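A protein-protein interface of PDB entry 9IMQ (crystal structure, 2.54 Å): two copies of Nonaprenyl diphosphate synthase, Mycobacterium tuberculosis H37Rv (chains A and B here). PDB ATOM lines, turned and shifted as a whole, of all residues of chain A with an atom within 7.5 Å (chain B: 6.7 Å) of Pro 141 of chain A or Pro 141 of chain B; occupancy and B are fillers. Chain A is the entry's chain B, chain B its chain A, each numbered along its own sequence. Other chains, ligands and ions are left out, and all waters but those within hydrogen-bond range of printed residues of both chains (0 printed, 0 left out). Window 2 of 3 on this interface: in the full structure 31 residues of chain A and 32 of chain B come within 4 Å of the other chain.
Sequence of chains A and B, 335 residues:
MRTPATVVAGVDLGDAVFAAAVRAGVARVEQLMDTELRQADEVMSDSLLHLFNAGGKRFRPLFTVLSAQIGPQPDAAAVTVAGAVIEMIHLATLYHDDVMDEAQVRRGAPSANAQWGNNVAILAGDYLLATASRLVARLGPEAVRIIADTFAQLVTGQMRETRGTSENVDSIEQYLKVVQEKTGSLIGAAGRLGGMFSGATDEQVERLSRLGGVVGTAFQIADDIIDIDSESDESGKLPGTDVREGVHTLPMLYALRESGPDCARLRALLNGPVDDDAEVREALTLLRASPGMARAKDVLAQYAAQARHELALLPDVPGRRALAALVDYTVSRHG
Among the printed residues, pairs that only touch across the chains: Ala 137 of chain A with Val 144 of chain B, Pro 141 of chain A with Ala 137 of chain B, Pro 141 of chain A with Pro 141 of chain B, Val 144 of chain A with Ser 133 of chain B, Val 144 of chain A with Ala 137 of chain B and Val 144 of chain A with Val 144 of chain B.
Ala 137 of chain A touches Val 144 of chain B, and with the chains exchanged Val 144 of chain A touches Ala 137 of chain B. Pro 141 of chain A touches Ala 137 of chain B, but with the chains exchanged Ala 137 of chain A does not touch Pro 141 of chain B (5.3 Å). Pro 141 of chain A touches its own counterpart, Pro 141 of chain B. Val 144 of chain A touches its own counterpart, Val 144 of chain B. Positions printed for both chains: 136, 137, 138, 139, 140, 141, 142, 143, 144, 145 and 146. Of the 7 pairs that touch across the chains among the printed residues, 4 have their exchanged pair printed and touching as well.
The guanidinium group (NH2) of Arg 145 of chain A is in hydrogen-bond range of the backbone carbonyl oxygen (O) of Ala 137 of chain B (3.3 Å).
Of the 12 printed residues of chain B, 4 touch a printed residue of chain A. Printed residues of chain B that touch a printed residue of chain A: Ser 133, Ala 137, Pro 141 and Val 144. Hydrophobic or aromatic side chains of chain B that line the printed part of chain A: Ala 137 and Val 144. Among the printed residues, 7 pairs touch across the chains.
Pro 141 of chain A touches just these residues of chain B: Ala 137 (3.7 Å) and Pro 141 (3.8 Å). Pro 141 of chain B touches just one residue of chain A: Pro 141. Of the printed residues of chain A, Val 144 of chain B touches Ala 137 and Val 144. Of the printed residues of chain B, Arg 145 of chain A touches Ala 137. Of the printed residues of chain B, Ala 137 of chain A touches Val 144. Of the printed residues of chain A, Ala 137 of chain B touches Pro 141, Val 144 and Arg 145. Arg 145 of chain B touches none of the printed residues of chain A.
OE1 of Glu 142 of chain A lies within salt-bridge range of NH1 of Arg 145 of chain A (3.7 Å).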
ATOM      1  N   VAL A 136      -6.810 -10.687  24.829  1.00  0.00           N
ATOM      2  CA  VAL A 136      -7.101 -10.746  23.403  1.00  0.00           C
ATOM      3  C   VAL A 136      -6.930 -12.164  22.890  1.00  0.00           C
ATOM      4  O   VAL A 136      -7.598 -12.558  21.918  1.00  0.00           O
ATOM      5  CB  VAL A 136      -6.234  -9.755  22.601  1.00  0.00           C
ATOM      6  CG1 VAL A 136      -4.927 -10.380  22.210  1.00  0.00           C
ATOM      7  CG2 VAL A 136      -6.981  -9.308  21.343  1.00  0.00           C
ATOM      8  N   ALA A 137      -6.057 -12.957  23.532  1.00  0.00           N
ATOM      9  CA  ALA A 137      -5.924 -14.362  23.154  1.00  0.00           C
ATOM     10  C   ALA A 137      -7.250 -15.092  23.262  1.00  0.00           C
ATOM     11  O   ALA A 137      -7.522 -15.994  22.458  1.00  0.00           O
ATOM     12  CB  ALA A 137      -4.876 -15.063  24.018  1.00  0.00           C
ATOM     13  N   ARG A 138      -8.088 -14.715  24.239  1.00  0.00           N
ATOM     14  CA  ARG A 138      -9.428 -15.290  24.327  1.00  0.00           C
ATOM     15  C   ARG A 138     -10.327 -14.814  23.193  1.00  0.00           C
ATOM     16  O   ARG A 138     -11.169 -15.579  22.722  1.00  0.00           O
ATOM     17  CB  ARG A 138     -10.058 -14.954  25.671  1.00  0.00           C
ATOM     18  CG  ARG A 138      -9.020 -14.779  26.751  1.00  0.00           C
ATOM     19  CD  ARG A 138      -9.553 -13.927  27.887  1.00  0.00           C
ATOM     20  NE  ARG A 138     -10.635 -14.602  28.587  1.00  0.00           N
ATOM     21  CZ  ARG A 138     -10.819 -14.550  29.896  1.00  0.00           C
ATOM     22  NH1 ARG A 138     -10.018 -13.838  30.678  1.00  0.00           N
ATOM     23  NH2 ARG A 138     -11.820 -15.246  30.436  1.00  0.00           N
ATOM     24  N   LEU A 139     -10.164 -13.566  22.745  1.00  0.00           N
ATOM     25  CA  LEU A 139     -10.924 -13.048  21.610  1.00  0.00           C
ATOM     26  C   LEU A 139     -10.525 -13.682  20.273  1.00  0.00           C
ATOM     27  O   LEU A 139     -11.238 -13.480  19.279  1.00  0.00           O
ATOM     28  CB  LEU A 139     -10.772 -11.522  21.522  1.00  0.00           C
ATOM     29  CG  LEU A 139     -11.461 -10.685  22.611  1.00  0.00           C
ATOM     30  CD1 LEU A 139     -11.084  -9.188  22.535  1.00  0.00           C
ATOM     31  CD2 LEU A 139     -12.985 -10.883  22.567  1.00  0.00           C
ATOM     32  N   GLY A 140      -9.403 -14.408  20.212  1.00  0.00           N
ATOM     33  CA  GLY A 140      -9.060 -15.187  19.044  1.00  0.00           C
ATOM     34  C   GLY A 140      -8.059 -14.545  18.095  1.00  0.00           C
ATOM     35  O   GLY A 140      -7.791 -13.335  18.135  1.00  0.00           O
ATOM     36  N   PRO A 141      -7.517 -15.363  17.184  1.00  0.00           N
ATOM     37  CA  PRO A 141      -6.416 -14.893  16.324  1.00  0.00           C
ATOM     38  C   PRO A 141      -6.755 -13.693  15.444  1.00  0.00           C
ATOM     39  O   PRO A 141      -5.869 -12.867  15.189  1.00  0.00           O
ATOM     40  CB  PRO A 141      -6.087 -16.132  15.479  1.00  0.00           C
ATOM     41  CG  PRO A 141      -6.530 -17.289  16.323  1.00  0.00           C
ATOM     42  CD  PRO A 141      -7.787 -16.799  17.002  1.00  0.00           C
ATOM     43  N   GLU A 142      -7.987 -13.558  14.949  1.00  0.00           N
ATOM     44  CA  GLU A 142      -8.270 -12.358  14.158  1.00  0.00           C
ATOM     45  C   GLU A 142      -8.245 -11.115  15.036  1.00  0.00           C
ATOM     46  O   GLU A 142      -7.735 -10.070  14.619  1.00  0.00           O
ATOM     47  CB  GLU A 142      -9.608 -12.465  13.429  1.00  0.00           C
ATOM     48  CG  GLU A 142      -9.946 -11.223  12.573  1.00  0.00           C
ATOM     49  CD  GLU A 142      -8.913 -10.946  11.465  1.00  0.00           C
ATOM     50  OE1 GLU A 142      -8.742 -11.824  10.590  1.00  0.00           O
ATOM     51  OE2 GLU A 142      -8.283  -9.853  11.450  1.00  0.00           O
ATOM     52  N   ALA A 143      -8.766 -11.218  16.263  1.00  0.00           N
ATOM     53  CA  ALA A 143      -8.646 -10.130  17.225  1.00  0.00           C
ATOM     54  C   ALA A 143      -7.208  -9.936  17.682  1.00  0.00           C
ATOM     55  O   ALA A 143      -6.856  -8.844  18.140  1.00  0.00           O
ATOM     56  CB  ALA A 143      -9.547 -10.384  18.432  1.00  0.00           C
ATOM     57  N   VAL A 144      -6.364 -10.965  17.557  1.00  0.00           N
ATOM     58  CA  VAL A 144      -4.946 -10.787  17.858  1.00  0.00           C
ATOM     59  C   VAL A 144      -4.252 -10.013  16.737  1.00  0.00           C
ATOM     60  O   VAL A 144      -3.477  -9.088  17.001  1.00  0.00           O
ATOM     61  CB  VAL A 144      -4.262 -12.144  18.132  1.00  0.00           C
ATOM     62  CG1 VAL A 144      -2.759 -11.951  18.317  1.00  0.00           C
ATOM     63  CG2 VAL A 144      -4.860 -12.811  19.376  1.00  0.00           C
ATOM     64  N   ARG A 145      -4.510 -10.379  15.474  1.00  0.00           N
ATOM     65  CA  ARG A 145      -3.959  -9.615  14.352  1.00  0.00           C
ATOM     66  C   ARG A 145      -4.340  -8.141  14.437  1.00  0.00           C
ATOM     67  O   ARG A 145      -3.499  -7.260  14.205  1.00  0.00           O
ATOM     68  CB  ARG A 145      -4.436 -10.195  13.022  1.00  0.00           C
ATOM     69  CG  ARG A 145      -3.876 -11.566  12.719  1.00  0.00           C
ATOM     70  CD  ARG A 145      -4.702 -12.300  11.655  1.00  0.00           C
ATOM     71  NE  ARG A 145      -4.269 -13.688  11.502  1.00  0.00           N
ATOM     72  CZ  ARG A 145      -5.095 -14.718  11.368  1.00  0.00           C
ATOM     73  NH1 ARG A 145      -6.410 -14.549  11.309  1.00  0.00           N
ATOM     74  NH2 ARG A 145      -4.589 -15.947  11.284  1.00  0.00           N
ATOM     75  N   ILE A 146      -5.601  -7.851  14.778  1.00  0.00           N
ATOM     76  CA  ILE A 146      -6.057  -6.463  14.832  1.00  0.00           C
ATOM     77  C   ILE A 146      -5.264  -5.686  15.876  1.00  0.00           C
ATOM     78  O   ILE A 146      -4.756  -4.591  15.607  1.00  0.00           O
ATOM     79  CB  ILE A 146      -7.568  -6.396  15.119  1.00  0.00           C
ATOM     80  CG1 ILE A 146      -8.376  -6.788  13.893  1.00  0.00           C
ATOM     81  CG2 ILE A 146      -7.976  -5.009  15.560  1.00  0.00           C
ATOM     82  CD1 ILE A 146      -9.710  -7.406  14.237  1.00  0.00           C
ATOM     83  N   ILE A 147      -5.149  -6.243  17.082  1.00  0.00           N
ATOM     84  CA  ILE A 147      -4.527  -5.513  18.179  1.00  0.00           C
ATOM     85  C   ILE A 147      -3.034  -5.388  17.945  1.00  0.00           C
ATOM     86  O   ILE A 147      -2.435  -4.335  18.193  1.00  0.00           O
ATOM     87  CB  ILE A 147      -4.835  -6.205  19.514  1.00  0.00           C
ATOM     88  CG1 ILE A 147      -6.292  -5.989  19.910  1.00  0.00           C
ATOM     89  CG2 ILE A 147      -3.914  -5.688  20.593  1.00  0.00           C
ATOM     90  CD1 ILE A 147      -6.674  -4.520  19.969  1.00  0.00           C
ATOM     91  N   SER B 133       3.368 -10.734  18.365  1.00  0.00           N
ATOM     92  CA  SER B 133       1.924 -10.924  18.459  1.00  0.00           C
ATOM     93  C   SER B 133       1.317 -11.225  17.092  1.00  0.00           C
ATOM     94  O   SER B 133       0.525 -12.158  16.937  1.00  0.00           O
ATOM     95  CB  SER B 133       1.276  -9.679  19.065  1.00  0.00           C
ATOM     96  OG  SER B 133       1.641  -9.516  20.431  1.00  0.00           O
ATOM     97  N   VAL B 136       2.421 -14.691  15.800  1.00  0.00           N
ATOM     98  CA  VAL B 136       1.905 -15.866  16.499  1.00  0.00           C
ATOM     99  C   VAL B 136       0.452 -16.137  16.127  1.00  0.00           C
ATOM    100  O   VAL B 136       0.013 -17.299  16.108  1.00  0.00           O
ATOM    101  CB  VAL B 136       2.079 -15.718  18.021  1.00  0.00           C
ATOM    102  CG1 VAL B 136       1.132 -14.666  18.569  1.00  0.00           C
ATOM    103  CG2 VAL B 136       1.814 -17.034  18.679  1.00  0.00           C
ATOM    104  N   ALA B 137      -0.312 -15.092  15.807  1.00  0.00           N
ATOM    105  CA  ALA B 137      -1.694 -15.301  15.392  1.00  0.00           C
ATOM    106  C   ALA B 137      -1.793 -16.186  14.150  1.00  0.00           C
ATOM    107  O   ALA B 137      -2.822 -16.832  13.947  1.00  0.00           O
ATOM    108  CB  ALA B 137      -2.385 -13.961  15.147  1.00  0.00           C
ATOM    109  N   ARG B 138      -0.744 -16.240  13.323  1.00  0.00           N
ATOM    110  CA  ARG B 138      -0.762 -17.131  12.169  1.00  0.00           C
ATOM    111  C   ARG B 138      -0.849 -18.597  12.591  1.00  0.00           C
ATOM    112  O   ARG B 138      -1.407 -19.423  11.857  1.00  0.00           O
ATOM    113  CB  ARG B 138       0.484 -16.898  11.307  1.00  0.00           C
ATOM    114  CG  ARG B 138       0.730 -15.442  10.921  1.00  0.00           C
ATOM    115  CD  ARG B 138       2.060 -15.182  10.155  1.00  0.00           C
ATOM    116  NE  ARG B 138       2.526 -16.304   9.350  1.00  0.00           N
ATOM    117  CZ  ARG B 138       3.573 -16.267   8.531  1.00  0.00           C
ATOM    118  NH1 ARG B 138       4.282 -15.163   8.361  1.00  0.00           N
ATOM    119  NH2 ARG B 138       3.911 -17.366   7.856  1.00  0.00           N
ATOM    120  N   LEU B 139      -0.339 -18.934  13.777  1.00  0.00           N
ATOM    121  CA  LEU B 139      -0.165 -20.324  14.185  1.00  0.00           C
ATOM    122  C   LEU B 139      -1.394 -20.932  14.846  1.00  0.00           C
ATOM    123  O   LEU B 139      -1.363 -22.124  15.180  1.00  0.00           O
ATOM    124  CB  LEU B 139       1.028 -20.468  15.144  1.00  0.00           C
ATOM    125  CG  LEU B 139       2.397 -20.077  14.590  1.00  0.00           C
ATOM    126  CD1 LEU B 139       3.470 -20.477  15.577  1.00  0.00           C
ATOM    127  CD2 LEU B 139       2.645 -20.714  13.236  1.00  0.00           C
ATOM    128  N   GLY B 140      -2.457 -20.166  15.056  1.00  0.00           N
ATOM    129  CA  GLY B 140      -3.661 -20.731  15.608  1.00  0.00           C
ATOM    130  C   GLY B 140      -3.951 -20.331  17.041  1.00  0.00           C
ATOM    131  O   GLY B 140      -3.099 -19.788  17.757  1.00  0.00           O
ATOM    132  N   PRO B 141      -5.185 -20.620  17.485  1.00  0.00           N
ATOM    133  CA  PRO B 141      -5.613 -20.189  18.827  1.00  0.00           C
ATOM    134  C   PRO B 141      -4.744 -20.719  19.942  1.00  0.00           C
ATOM    135  O   PRO B 141      -4.486 -20.004  20.920  1.00  0.00           O
ATOM    136  CB  PRO B 141      -7.041 -20.751  18.940  1.00  0.00           C
ATOM    137  CG  PRO B 141      -7.449 -21.079  17.570  1.00  0.00           C
ATOM    138  CD  PRO B 141      -6.213 -21.430  16.810  1.00  0.00           C
ATOM    139  N   GLU B 142      -4.306 -21.975  19.845  1.00  0.00           N
ATOM    140  CA  GLU B 142      -3.564 -22.537  20.964  1.00  0.00           C
ATOM    141  C   GLU B 142      -2.161 -21.954  21.043  1.00  0.00           C
ATOM    142  O   GLU B 142      -1.687 -21.627  22.139  1.00  0.00           O
ATOM    143  CB  GLU B 142      -3.519 -24.055  20.877  1.00  0.00           C
ATOM    144  CG  GLU B 142      -3.308 -24.664  22.244  1.00  0.00           C
ATOM    145  CD  GLU B 142      -2.903 -26.101  22.159  1.00  0.00           C
ATOM    146  OE1 GLU B 142      -3.210 -26.725  21.113  1.00  0.00           O
ATOM    147  OE2 GLU B 142      -2.270 -26.591  23.126  1.00  0.00           O
ATOM    148  N   ALA B 143      -1.487 -21.806  19.896  1.00  0.00           N
ATOM    149  CA  ALA B 143      -0.195 -21.124  19.887  1.00  0.00           C
ATOM    150  C   ALA B 143      -0.320 -19.725  20.471  1.00  0.00           C
ATOM    151  O   ALA B 143       0.542 -19.286  21.244  1.00  0.00           O
ATOM    152  CB  ALA B 143       0.357 -21.046  18.466  1.00  0.00           C
ATOM    153  N   VAL B 144      -1.399 -19.019  20.112  1.00  0.00           N
ATOM    154  CA  VAL B 144      -1.649 -17.690  20.651  1.00  0.00           C
ATOM    155  C   VAL B 144      -1.773 -17.746  22.166  1.00  0.00           C
ATOM    156  O   VAL B 144      -1.166 -16.946  22.882  1.00  0.00           O
ATOM    157  CB  VAL B 144      -2.902 -17.080  19.998  1.00  0.00           C
ATOM    158  CG1 VAL B 144      -3.415 -15.926  20.814  1.00  0.00           C
ATOM    159  CG2 VAL B 144      -2.576 -16.635  18.599  1.00  0.00           C
ATOM    160  N   ARG B 145      -2.567 -18.681  22.682  1.00  0.00           N
ATOM    161  CA  ARG B 145      -2.684 -18.798  24.134  1.00  0.00           C
ATOM    162  C   ARG B 145      -1.326 -19.085  24.774  1.00  0.00           C
ATOM    163  O   ARG B 145      -0.975 -18.491  25.802  1.00  0.00           O
ATOM    164  CB  ARG B 145      -3.688 -19.888  24.491  1.00  0.00           C
ATOM    165  CG  ARG B 145      -5.135 -19.482  24.288  1.00  0.00           C
ATOM    166  CD  ARG B 145      -6.080 -20.229  25.267  1.00  0.00           C
ATOM    167  NE  ARG B 145      -6.047 -21.685  25.123  1.00  0.00           N
ATOM    168  CZ  ARG B 145      -6.376 -22.353  24.021  1.00  0.00           C
ATOM    169  NH1 ARG B 145      -6.868 -21.736  22.950  1.00  0.00           N
ATOM    170  NH2 ARG B 145      -6.209 -23.675  23.991  1.00  0.00           N
ATOM    171  N   ILE B 146      -0.537 -19.973  24.160  1.00  0.00           N
ATOM    172  CA  ILE B 146       0.770 -20.322  24.709  1.00  0.00           C
ATOM    173  C   ILE B 146       1.631 -19.072  24.868  1.00  0.00           C
ATOM    174  O   ILE B 146       2.137 -18.782  25.960  1.00  0.00           O
ATOM    175  CB  ILE B 146       1.464 -21.384  23.831  1.00  0.00           C
ATOM    176  CG1 ILE B 146       0.887 -22.766  24.100  1.00  0.00           C
ATOM    177  CG2 ILE B 146       2.958 -21.439  24.102  1.00  0.00           C
ATOM    178  CD1 ILE B 146       0.885 -23.632  22.871  1.00  0.00           C
